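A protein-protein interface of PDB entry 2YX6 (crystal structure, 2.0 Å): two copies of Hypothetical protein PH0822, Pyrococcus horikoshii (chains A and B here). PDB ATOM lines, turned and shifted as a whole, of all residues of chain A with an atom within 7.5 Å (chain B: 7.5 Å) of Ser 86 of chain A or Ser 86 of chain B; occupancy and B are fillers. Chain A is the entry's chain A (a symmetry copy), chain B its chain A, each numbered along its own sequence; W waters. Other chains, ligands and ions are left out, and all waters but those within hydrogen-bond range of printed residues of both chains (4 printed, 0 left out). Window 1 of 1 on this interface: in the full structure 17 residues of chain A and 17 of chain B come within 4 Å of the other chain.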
ATOM      1  N   ALA A   4       5.420   1.545  12.786  1.00  0.00           N
ATOM      2  CA  ALA A   4       4.770   0.993  13.979  1.00  0.00           C
ATOM      3  C   ALA A   4       4.413   2.125  14.977  1.00  0.00           C
ATOM      4  O   ALA A   4       5.230   2.971  15.231  1.00  0.00           O
ATOM      5  CB  ALA A   4       5.750   0.039  14.665  1.00  0.00           C
ATOM      6  N   ILE A  59       8.158  -5.783  17.386  1.00  0.00           N
ATOM      7  CA  ILE A  59       8.112  -4.794  16.283  1.00  0.00           C
ATOM      8  C   ILE A  59       8.942  -5.234  15.056  1.00  0.00           C
ATOM      9  O   ILE A  59       8.419  -5.298  13.949  1.00  0.00           O
ATOM     10  CB  ILE A  59       8.466  -3.382  16.831  1.00  0.00           C
ATOM     11  CG1 ILE A  59       7.434  -2.976  17.874  1.00  0.00           C
ATOM     12  CG2 ILE A  59       8.535  -2.375  15.741  1.00  0.00           C
ATOM     13  CD1 ILE A  59       5.966  -2.977  17.307  1.00  0.00           C
ATOM     14  N   ALA A  64       8.507  -3.673  10.969  1.00  0.00           N
ATOM     15  CA  ALA A  64       8.465  -2.196  11.092  1.00  0.00           C
ATOM     16  C   ALA A  64       9.896  -1.711  11.170  1.00  0.00           C
ATOM     17  O   ALA A  64      10.731  -2.339  11.840  1.00  0.00           O
ATOM     18  CB  ALA A  64       7.680  -1.785  12.274  1.00  0.00           C
ATOM     19  N   LYS A  65      10.220  -0.635  10.451  1.00  0.00           N
ATOM     20  CA  LYS A  65      11.588  -0.132  10.491  1.00  0.00           C
ATOM     21  C   LYS A  65      11.615   1.227  11.166  1.00  0.00           C
ATOM     22  O   LYS A  65      12.666   1.732  11.519  1.00  0.00           O
ATOM     23  CB  LYS A  65      12.154  -0.014   9.059  1.00  0.00           C
ATOM     24  CG  LYS A  65      12.115  -1.357   8.273  1.00  0.00           C
ATOM     25  CD  LYS A  65      13.355  -1.503   7.383  1.00  0.00           C
ATOM     26  CE  LYS A  65      14.606  -1.662   8.223  1.00  0.00           C
ATOM     27  NZ  LYS A  65      14.403  -2.825   9.156  1.00  0.00           N
ATOM     28  N   ILE A  66      10.435   1.799  11.373  1.00  0.00           N
ATOM     29  CA  ILE A  66      10.322   3.045  12.135  1.00  0.00           C
ATOM     30  C   ILE A  66       9.227   2.916  13.191  1.00  0.00           C
ATOM     31  O   ILE A  66       8.206   2.335  12.965  1.00  0.00           O
ATOM     32  CB  ILE A  66      10.004   4.262  11.215  1.00  0.00           C
ATOM     33  CG1 ILE A  66      11.127   4.429  10.202  1.00  0.00           C
ATOM     34  CG2 ILE A  66       9.796   5.552  12.071  1.00  0.00           C
ATOM     35  CD1 ILE A  66      11.100   5.749   9.455  1.00  0.00           C
ATOM     36  N   VAL A  67       9.474   3.465  14.365  1.00  0.00           N
ATOM     37  CA  VAL A  67       8.486   3.487  15.448  1.00  0.00           C
ATOM     38  C   VAL A  67       8.221   4.944  15.820  1.00  0.00           C
ATOM     39  O   VAL A  67       9.182   5.701  16.090  1.00  0.00           O
ATOM     40  CB  VAL A  67       9.040   2.727  16.668  1.00  0.00           C
ATOM     41  CG1 VAL A  67       8.116   2.885  17.868  1.00  0.00           C
ATOM     42  CG2 VAL A  67       9.303   1.267  16.310  1.00  0.00           C
ATOM     43  N   LEU A  68       6.948   5.328  15.849  1.00  0.00           N
ATOM     44  CA  LEU A  68       6.569   6.636  16.322  1.00  0.00           C
ATOM     45  C   LEU A  68       5.985   6.516  17.693  1.00  0.00           C
ATOM     46  O   LEU A  68       4.968   5.879  17.841  1.00  0.00           O
ATOM     47  CB  LEU A  68       5.498   7.281  15.418  1.00  0.00           C
ATOM     48  CG  LEU A  68       5.929   7.324  13.919  1.00  0.00           C
ATOM     49  CD1 LEU A  68       4.805   7.914  13.097  1.00  0.00           C
ATOM     50  CD2 LEU A  68       7.266   8.156  13.732  1.00  0.00           C
ATOM     51  N   ILE A  77      14.797   2.448  23.244  1.00  0.00           N
ATOM     52  CA  ILE A  77      15.299   3.165  22.064  1.00  0.00           C
ATOM     53  C   ILE A  77      16.595   2.516  21.660  1.00  0.00           C
ATOM     54  O   ILE A  77      16.773   2.170  20.518  1.00  0.00           O
ATOM     55  CB  ILE A  77      15.616   4.722  22.349  1.00  0.00           C
ATOM     56  CG1 ILE A  77      14.327   5.556  22.447  1.00  0.00           C
ATOM     57  CG2 ILE A  77      16.445   5.325  21.211  1.00  0.00           C
ATOM     58  CD1 ILE A  77      14.479   6.941  23.117  1.00  0.00           C
ATOM     59  N   PHE A  80      16.060  -0.815  20.135  1.00  0.00           N
ATOM     60  CA  PHE A  80      15.469  -0.640  18.813  1.00  0.00           C
ATOM     61  C   PHE A  80      16.565  -0.343  17.803  1.00  0.00           C
ATOM     62  O   PHE A  80      16.652  -0.959  16.719  1.00  0.00           O
ATOM     63  CB  PHE A  80      14.416   0.478  18.806  1.00  0.00           C
ATOM     64  CG  PHE A  80      12.989   0.022  19.101  1.00  0.00           C
ATOM     65  CD1 PHE A  80      12.303   0.507  20.211  1.00  0.00           C
ATOM     66  CD2 PHE A  80      12.345  -0.878  18.287  1.00  0.00           C
ATOM     67  CE1 PHE A  80      11.019   0.103  20.485  1.00  0.00           C
ATOM     68  CE2 PHE A  80      11.045  -1.295  18.531  1.00  0.00           C
ATOM     69  CZ  PHE A  80      10.374  -0.830  19.625  1.00  0.00           C
ATOM     70  N   ASN A  81      17.430   0.586  18.181  1.00  0.00           N
ATOM     71  CA  ASN A  81      18.507   1.013  17.373  1.00  0.00           C
ATOM     72  C   ASN A  81      19.477  -0.129  17.054  1.00  0.00           C
ATOM     73  O   ASN A  81      19.967  -0.241  15.924  1.00  0.00           O
ATOM     74  CB  ASN A  81      19.198   2.169  18.105  1.00  0.00           C
ATOM     75  CG  ASN A  81      18.434   3.505  17.963  1.00  0.00           C
ATOM     76  OD1 ASN A  81      17.363   3.594  17.326  1.00  0.00           O
ATOM     77  ND2 ASN A  81      18.977   4.529  18.597  1.00  0.00           N
ATOM     78  N   LEU A  83      18.671  -3.065  16.625  1.00  0.00           N
ATOM     79  CA  LEU A  83      17.932  -3.893  15.654  1.00  0.00           C
ATOM     80  C   LEU A  83      17.680  -3.133  14.341  1.00  0.00           C
ATOM     81  O   LEU A  83      16.891  -3.559  13.456  1.00  0.00           O
ATOM     82  CB  LEU A  83      16.618  -4.279  16.288  1.00  0.00           C
ATOM     83  CG  LEU A  83      16.690  -5.219  17.515  1.00  0.00           C
ATOM     84  CD1 LEU A  83      15.251  -5.574  17.835  1.00  0.00           C
ATOM     85  CD2 LEU A  83      17.542  -6.506  17.284  1.00  0.00           C
ATOM     86  N   GLY A  84      18.324  -1.981  14.220  1.00  0.00           N
ATOM     87  CA  GLY A  84      18.296  -1.228  12.935  1.00  0.00           C
ATOM     88  C   GLY A  84      16.945  -0.575  12.816  1.00  0.00           C
ATOM     89  O   GLY A  84      16.480  -0.313  11.701  1.00  0.00           O
ATOM     90  N   ILE A  85      16.285  -0.360  13.957  1.00  0.00           N
ATOM     91  CA  ILE A  85      14.984   0.322  13.979  1.00  0.00           C
ATOM     92  C   ILE A  85      15.080   1.745  14.614  1.00  0.00           C
ATOM     93  O   ILE A  85      15.701   1.913  15.655  1.00  0.00           O
ATOM     94  CB  ILE A  85      13.913  -0.534  14.673  1.00  0.00           C
ATOM     95  CG1 ILE A  85      13.733  -1.910  13.988  1.00  0.00           C
ATOM     96  CG2 ILE A  85      12.591   0.180  14.746  1.00  0.00           C
ATOM     97  CD1 ILE A  85      12.738  -2.716  14.728  1.00  0.00           C
ATOM     98  N   SER A  86      14.493   2.728  13.940  1.00  0.00           N
ATOM     99  CA  SER A  86      14.592   4.136  14.317  1.00  0.00           C
ATOM    100  C   SER A  86      13.390   4.455  15.111  1.00  0.00           C
ATOM    101  O   SER A  86      12.329   3.962  14.810  1.00  0.00           O
ATOM    102  CB  SER A  86      14.555   5.025  13.052  1.00  0.00           C
ATOM    103  OG  SER A  86      15.696   4.670  12.312  1.00  0.00           O
ATOM    104  N   VAL A  87      13.519   5.327  16.084  1.00  0.00           N
ATOM    105  CA  VAL A  87      12.390   5.635  16.948  1.00  0.00           C
ATOM    106  C   VAL A  87      12.197   7.159  16.884  1.00  0.00           C
ATOM    107  O   VAL A  87      13.192   7.899  16.963  1.00  0.00           O
ATOM    108  CB  VAL A  87      12.684   5.170  18.452  1.00  0.00           C
ATOM    109  CG1 VAL A  87      11.524   5.600  19.490  1.00  0.00           C
ATOM    110  CG2 VAL A  87      12.966   3.679  18.559  1.00  0.00           C
ATOM    111  N   VAL A  88      10.953   7.626  16.790  1.00  0.00           N
ATOM    112  CA  VAL A  88      10.628   9.049  16.934  1.00  0.00           C
ATOM    113  C   VAL A  88       9.822   9.227  18.233  1.00  0.00           C
ATOM    114  O   VAL A  88       8.828   8.500  18.447  1.00  0.00           O
ATOM    115  CB  VAL A  88       9.771   9.593  15.726  1.00  0.00           C
ATOM    116  CG1 VAL A  88       9.496  11.127  15.909  1.00  0.00           C
ATOM    117  CG2 VAL A  88      10.487   9.333  14.417  1.00  0.00           C
ATOM    118  N   PHE A 102       3.326  12.766   9.297  1.00  0.00           N
ATOM    119  CA  PHE A 102       4.566  12.063   9.021  1.00  0.00           C
ATOM    120  C   PHE A 102       4.933  12.051   7.496  1.00  0.00           C
ATOM    121  O   PHE A 102       6.031  12.451   7.068  1.00  0.00           O
ATOM    122  CB  PHE A 102       4.462  10.644   9.631  1.00  0.00           C
ATOM    123  CG  PHE A 102       5.739   9.857   9.511  1.00  0.00           C
ATOM    124  CD1 PHE A 102       6.801  10.098  10.391  1.00  0.00           C
ATOM    125  CD2 PHE A 102       5.903   8.922   8.466  1.00  0.00           C
ATOM    126  CE1 PHE A 102       8.029   9.385  10.240  1.00  0.00           C
ATOM    127  CE2 PHE A 102       7.094   8.233   8.315  1.00  0.00           C
ATOM    128  CZ  PHE A 102       8.157   8.466   9.199  1.00  0.00           C
ATOM    129  N   LEU A 107       5.646  16.914  11.348  1.00  0.00           N
ATOM    130  CA  LEU A 107       5.168  16.164  12.464  1.00  0.00           C
ATOM    131  C   LEU A 107       5.123  17.161  13.611  1.00  0.00           C
ATOM    132  O   LEU A 107       5.996  18.034  13.692  1.00  0.00           O
ATOM    133  CB  LEU A 107       6.126  14.993  12.711  1.00  0.00           C
ATOM    134  CG  LEU A 107       5.545  13.680  13.153  1.00  0.00           C
ATOM    135  CD1 LEU A 107       4.454  13.418  12.221  1.00  0.00           C
ATOM    136  CD2 LEU A 107       6.601  12.602  13.059  1.00  0.00           C
ATOM    137  N   ALA B   4      20.636   8.647   5.247  1.00  0.00           N
ATOM    138  CA  ALA B   4      21.661   9.695   5.278  1.00  0.00           C
ATOM    139  C   ALA B   4      22.674   9.432   6.422  1.00  0.00           C
ATOM    140  O   ALA B   4      22.269   9.131   7.515  1.00  0.00           O
ATOM    141  CB  ALA B   4      20.972  11.035   5.544  1.00  0.00           C
ATOM    142  N   ILE B  59      19.100  17.564   4.568  1.00  0.00           N
ATOM    143  CA  ILE B  59      18.797  16.114   4.532  1.00  0.00           C
ATOM    144  C   ILE B  59      17.406  15.812   3.929  1.00  0.00           C
ATOM    145  O   ILE B  59      17.299  15.041   2.981  1.00  0.00           O
ATOM    146  CB  ILE B  59      19.041  15.494   5.938  1.00  0.00           C
ATOM    147  CG1 ILE B  59      20.507  15.663   6.312  1.00  0.00           C
ATOM    148  CG2 ILE B  59      18.650  14.061   5.978  1.00  0.00           C
ATOM    149  CD1 ILE B  59      21.479  15.008   5.263  1.00  0.00           C
ATOM    150  N   ALA B  64      16.095  11.938   2.315  1.00  0.00           N
ATOM    151  CA  ALA B  64      16.483  10.918   3.319  1.00  0.00           C
ATOM    152  C   ALA B  64      15.398  10.893   4.374  1.00  0.00           C
ATOM    153  O   ALA B  64      14.890  11.953   4.771  1.00  0.00           O
ATOM    154  CB  ALA B  64      17.806  11.221   3.899  1.00  0.00           C
ATOM    155  N   LYS B  65      14.985   9.699   4.801  1.00  0.00           N
ATOM    156  CA  LYS B  65      13.939   9.622   5.815  1.00  0.00           C
ATOM    157  C   LYS B  65      14.514   9.059   7.103  1.00  0.00           C
ATOM    158  O   LYS B  65      13.890   9.122   8.148  1.00  0.00           O
ATOM    159  CB  LYS B  65      12.784   8.724   5.323  1.00  0.00           C
ATOM    160  CG  LYS B  65      12.170   9.202   3.974  1.00  0.00           C
ATOM    161  CD  LYS B  65      10.652   8.980   3.959  1.00  0.00           C
ATOM    162  CE  LYS B  65       9.966   9.887   4.961  1.00  0.00           C
ATOM    163  NZ  LYS B  65      10.362  11.307   4.663  1.00  0.00           N
ATOM    164  N   ILE B  66      15.732   8.537   7.019  1.00  0.00           N
ATOM    165  CA  ILE B  66      16.444   8.086   8.216  1.00  0.00           C
ATOM    166  C   ILE B  66      17.865   8.646   8.223  1.00  0.00           C
ATOM    167  O   ILE B  66      18.509   8.727   7.217  1.00  0.00           O
ATOM    168  CB  ILE B  66      16.508   6.531   8.303  1.00  0.00           C
ATOM    169  CG1 ILE B  66      15.091   5.977   8.361  1.00  0.00           C
ATOM    170  CG2 ILE B  66      17.355   6.089   9.538  1.00  0.00           C
ATOM    171  CD1 ILE B  66      15.012   4.515   8.758  1.00  0.00           C
ATOM    172  N   VAL B  67      18.334   9.046   9.389  1.00  0.00           N
ATOM    173  CA  VAL B  67      19.706   9.533   9.561  1.00  0.00           C
ATOM    174  C   VAL B  67      20.401   8.645  10.590  1.00  0.00           C
ATOM    175  O   VAL B  67      19.863   8.449  11.705  1.00  0.00           O
ATOM    176  CB  VAL B  67      19.679  10.990  10.059  1.00  0.00           C
ATOM    177  CG1 VAL B  67      21.080  11.465  10.419  1.00  0.00           C
ATOM    178  CG2 VAL B  67      18.993  11.889   9.035  1.00  0.00           C
ATOM    179  N   LEU B  68      21.574   8.128  10.235  1.00  0.00           N
ATOM    180  CA  LEU B  68      22.384   7.392  11.172  1.00  0.00           C
ATOM    181  C   LEU B  68      23.525   8.249  11.620  1.00  0.00           C
ATOM    182  O   LEU B  68      24.337   8.614  10.800  1.00  0.00           O
ATOM    183  CB  LEU B  68      22.984   6.121  10.534  1.00  0.00           C
ATOM    184  CG  LEU B  68      21.895   5.209   9.888  1.00  0.00           C
ATOM    185  CD1 LEU B  68      22.568   4.021   9.237  1.00  0.00           C
ATOM    186  CD2 LEU B  68      20.831   4.737  10.964  1.00  0.00           C
ATOM    187  N   ILE B  77      17.925  16.571  16.558  1.00  0.00           N
ATOM    188  CA  ILE B  77      17.065  15.380  16.570  1.00  0.00           C
ATOM    189  C   ILE B  77      15.638  15.855  16.543  1.00  0.00           C
ATOM    190  O   ILE B  77      14.862  15.410  15.734  1.00  0.00           O
ATOM    191  CB  ILE B  77      17.242  14.476  17.895  1.00  0.00           C
ATOM    192  CG1 ILE B  77      18.551  13.670  17.863  1.00  0.00           C
ATOM    193  CG2 ILE B  77      16.102  13.462  18.017  1.00  0.00           C
ATOM    194  CD1 ILE B  77      19.021  13.108  19.225  1.00  0.00           C
ATOM    195  N   PHE B  80      14.694  17.227  13.237  1.00  0.00           N
ATOM    196  CA  PHE B  80      14.587  16.128  12.283  1.00  0.00           C
ATOM    197  C   PHE B  80      13.222  15.474  12.412  1.00  0.00           C
ATOM    198  O   PHE B  80      12.499  15.248  11.418  1.00  0.00           O
ATOM    199  CB  PHE B  80      15.701  15.090  12.486  1.00  0.00           C
ATOM    200  CG  PHE B  80      16.968  15.335  11.672  1.00  0.00           C
ATOM    201  CD1 PHE B  80      18.188  15.558  12.306  1.00  0.00           C
ATOM    202  CD2 PHE B  80      16.943  15.349  10.298  1.00  0.00           C
ATOM    203  CE1 PHE B  80      19.334  15.779  11.581  1.00  0.00           C
ATOM    204  CE2 PHE B  80      18.086  15.557   9.541  1.00  0.00           C
ATOM    205  CZ  PHE B  80      19.280  15.787  10.159  1.00  0.00           C
ATOM    206  N   ASN B  81      12.853  15.203  13.655  1.00  0.00           N
ATOM    207  CA  ASN B  81      11.628  14.579  13.978  1.00  0.00           C
ATOM    208  C   ASN B  81      10.421  15.408  13.526  1.00  0.00           C
ATOM    209  O   ASN B  81       9.432  14.859  13.025  1.00  0.00           O
ATOM    210  CB  ASN B  81      11.624  14.333  15.492  1.00  0.00           C
ATOM    211  CG  ASN B  81      12.469  13.105  15.896  1.00  0.00           C
ATOM    212  OD1 ASN B  81      13.088  12.416  15.057  1.00  0.00           O
ATOM    213  ND2 ASN B  81      12.518  12.864  17.195  1.00  0.00           N
ATOM    214  N   LEU B  83      10.319  17.141  10.989  1.00  0.00           N
ATOM    215  CA  LEU B  83      10.312  16.981   9.522  1.00  0.00           C
ATOM    216  C   LEU B  83      10.037  15.524   9.116  1.00  0.00           C
ATOM    217  O   LEU B  83      10.193  15.112   7.935  1.00  0.00           O
ATOM    218  CB  LEU B  83      11.663  17.415   9.008  1.00  0.00           C
ATOM    219  CG  LEU B  83      12.013  18.915   9.160  1.00  0.00           C
ATOM    220  CD1 LEU B  83      13.323  19.099   8.420  1.00  0.00           C
ATOM    221  CD2 LEU B  83      10.921  19.885   8.609  1.00  0.00           C
ATOM    222  N   GLY B  84       9.658  14.722  10.100  1.00  0.00           N
ATOM    223  CA  GLY B  84       9.204  13.332   9.815  1.00  0.00           C
ATOM    224  C   GLY B  84      10.426  12.506   9.507  1.00  0.00           C
ATOM    225  O   GLY B  84      10.330  11.502   8.793  1.00  0.00           O
ATOM    226  N   ILE B  85      11.584  12.952   9.998  1.00  0.00           N
ATOM    227  CA  ILE B  85      12.837  12.206   9.817  1.00  0.00           C
ATOM    228  C   ILE B  85      13.346  11.584  11.156  1.00  0.00           C
ATOM    229  O   ILE B  85      13.357  12.253  12.179  1.00  0.00           O
ATOM    230  CB  ILE B  85      13.918  13.075   9.153  1.00  0.00           C
ATOM    231  CG1 ILE B  85      13.466  13.613   7.774  1.00  0.00           C
ATOM    232  CG2 ILE B  85      15.218  12.334   9.013  1.00  0.00           C
ATOM    233  CD1 ILE B  85      14.513  14.490   7.207  1.00  0.00           C
ATOM    234  N   SER B  86      13.711  10.307  11.106  1.00  0.00           N
ATOM    235  CA  SER B  86      14.087   9.530  12.284  1.00  0.00           C
ATOM    236  C   SER B  86      15.560   9.568  12.373  1.00  0.00           C
ATOM    237  O   SER B  86      16.220   9.530  11.361  1.00  0.00           O
ATOM    238  CB  SER B  86      13.679   8.050  12.094  1.00  0.00           C
ATOM    239  OG  SER B  86      12.278   8.061  11.983  1.00  0.00           O
ATOM    240  N   VAL B  87      16.096   9.577  13.571  1.00  0.00           N
ATOM    241  CA  VAL B  87      17.538   9.684  13.729  1.00  0.00           C
ATOM    242  C   VAL B  87      17.972   8.479  14.581  1.00  0.00           C
ATOM    243  O   VAL B  87      17.310   8.179  15.588  1.00  0.00           O
ATOM    244  CB  VAL B  87      17.928  11.055  14.459  1.00  0.00           C
ATOM    245  CG1 VAL B  87      19.505  11.178  14.784  1.00  0.00           C
ATOM    246  CG2 VAL B  87      17.447  12.281  13.699  1.00  0.00           C
ATOM    247  N   VAL B  88      19.077   7.827  14.220  1.00  0.00           N
ATOM    248  CA  VAL B  88      19.705   6.805  15.064  1.00  0.00           C
ATOM    249  C   VAL B  88      21.058   7.353  15.553  1.00  0.00           C
ATOM    250  O   VAL B  88      21.864   7.831  14.726  1.00  0.00           O
ATOM    251  CB  VAL B  88      19.953   5.456  14.286  1.00  0.00           C
ATOM    252  CG1 VAL B  88      20.579   4.387  15.249  1.00  0.00           C
ATOM    253  CG2 VAL B  88      18.655   4.945  13.695  1.00  0.00           C
ATOM    254  N   PHE B 102      22.935  -2.304   9.404  1.00  0.00           N
ATOM    255  CA  PHE B 102      21.607  -1.718   9.392  1.00  0.00           C
ATOM    256  C   PHE B 102      20.550  -2.620   8.664  1.00  0.00           C
ATOM    257  O   PHE B 102      19.486  -2.975   9.204  1.00  0.00           O
ATOM    258  CB  PHE B 102      21.712  -0.297   8.786  1.00  0.00           C
ATOM    259  CG  PHE B 102      20.412   0.459   8.829  1.00  0.00           C
ATOM    260  CD1 PHE B 102      19.984   1.058  10.021  1.00  0.00           C
ATOM    261  CD2 PHE B 102      19.578   0.508   7.690  1.00  0.00           C
ATOM    262  CE1 PHE B 102      18.724   1.729  10.069  1.00  0.00           C
ATOM    263  CE2 PHE B 102      18.356   1.155   7.737  1.00  0.00           C
ATOM    264  CZ  PHE B 102      17.927   1.762   8.926  1.00  0.00           C
ATOM    265  N   LEU B 107      22.778  -3.588  14.416  1.00  0.00           N
ATOM    266  CA  LEU B 107      23.580  -2.408  14.358  1.00  0.00           C
ATOM    267  C   LEU B 107      24.373  -2.414  15.655  1.00  0.00           C
ATOM    268  O   LEU B 107      23.842  -2.835  16.690  1.00  0.00           O
ATOM    269  CB  LEU B 107      22.653  -1.196  14.215  1.00  0.00           C
ATOM    270  CG  LEU B 107      23.104  -0.056  13.346  1.00  0.00           C
ATOM    271  CD1 LEU B 107      23.527  -0.678  12.097  1.00  0.00           C
ATOM    272  CD2 LEU B 107      21.947   0.888  13.110  1.00  0.00           C
HETATM  273  O   HOH W   1       8.232  11.559   6.583  1.00  0.00           O
HETATM  274  O   HOH W   2      15.947   6.236  17.050  1.00  0.00           O
HETATM  275  O   HOH W   3      14.679  10.008  15.909  1.00  0.00           O
HETATM  276  O   HOH W   4      17.201  -2.194   9.413  1.00  0.00           O
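N of Val 88 of chain B lies within hydrogen-bond range of O of Val 67 of chain B (2.7 Å). O of Ile 66 of chain A lies within hydrogen-bond range of N of Ala 4 of chain A, at 2.9 Å. The backbone NH of Val 67 of chain B sits at hydrogen-bond distance from the backbone carbonyl oxygen of Ser 86 of chain B (2.9 Å). N of Val 67 of chain A sits at hydrogen-bond distance from O of Ser 86 of chain A (2.9 Å). The side-chain amide oxygen of Asn 81 of chain B lies close to the backbone carbonyl oxygen of Ile 85 of chain B (2.9 Å). N of Ala 4 of chain B lies within hydrogen-bond range of O of Ile 66 of chain B.
Among the printed residues, merely in contact across the chains: Ile 66 of chain A with Ser 86 of chain B, Asn 81 of chain A with Val 88 of chain B, Asn 81 of chain A with Leu 107 of chain B, Gly 84 of chain A with Phe 102 of chain B, Ser 86 of chain A with Ile 66 of chain B, Ser 86 of chain A with Ser 86 of chain B, Ser 86 of chain A with Val 88 of chain B, Val 88 of chain A with Asn 81 of chain B, Val 88 of chain A with Ser 86 of chain B, Phe 102 of chain A with Gly 84 of chain B and Leu 107 of chain A with Asn 81 of chain B.
Ser 86 of chain B touches three residues of chain A. Of the printed residues of chain B, Phe 102 of chain A touches Gly 84 (3.4 Å). Of the printed residues of chain A, Leu 107 of chain B touches Asn 81. Of the printed residues of chain B, Val 88 of chain A touches Asn 81 and Ser 86. Of the printed residues of chain B, Leu 107 of chain A touches Asn 81. Of the printed residues of chain A, Ile 66 of chain B touches Ser 86 (3.5 Å). Leu 68 of chain A touches none of the printed residues of chain B. Leu 68 of chain B touches none of the printed residues of chain A. The nearest residue of chain B that does not touch Ser 86 of chain A is Phe 102 of chain B (4.8 Å).
Of the 18 printed residues of chain B, 7 touch a printed residue of chain A. Hydrophobic or aromatic side chains of chain B that line the printed part of chain A: Ile 66, Val 88, Phe 102 and Leu 107. Of the 18 printed residues of chain A, 7 touch a printed residue of chain B. Hydrophobic or aromatic side chains of chain A within 4 Å of the printed part of chain B: Ile 66, Val 88, Phe 102 and Leu 107. Among the printed residues, no Asp or Glu carboxylate lies within 4 Å of a Lys or Arg side-chain nitrogen of the other chain.
Ile 66 of chain A touches Ser 86 of chain B, and with the chains exchanged Ser 86 of chain A touches Ile 66 of chain B. Asn 81 of chain A touches Leu 107 of chain B, and with the chains exchanged Leu 107 of chain A touches Asn 81 of chain B. Gly 84 of chain A touches Phe 102 of chain B, and with the chains exchanged Phe 102 of chain A touches Gly 84 of chain B. Ser 86 of chain B touches its own counterpart, Ser 86 of chain A. 18 positions are printed for both chains. Of the 11 pairs that touch across the chains among the printed residues, 11 have their exchanged pair printed and touching as well.
Water W4 lies within hydrogen-bond range of O of Phe 102 of chain B (2.4 Å), NZ of Lys 65 of chain A (2.9 Å) and O of Gly 84 of chain A (3.0 Å). Water W1 lies within hydrogen-bond range of O of Phe 102 of chain A (2.4 Å), NZ of Lys 65 of chain B (2.9 Å) and O of Gly 84 of chain B (3.0 Å). Water W2 lies within hydrogen-bond range of N of Val 87 of chain A, O of Val 87 of chain B and OD1 of Asn 81 of chain A. Water W3 lies within hydrogen-bond range of N of Val 87 of chain B (2.8 Å), O of Val 87 of chain A (2.8 Å) and OD1 of Asn 81 of chain B (3.0 Å).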
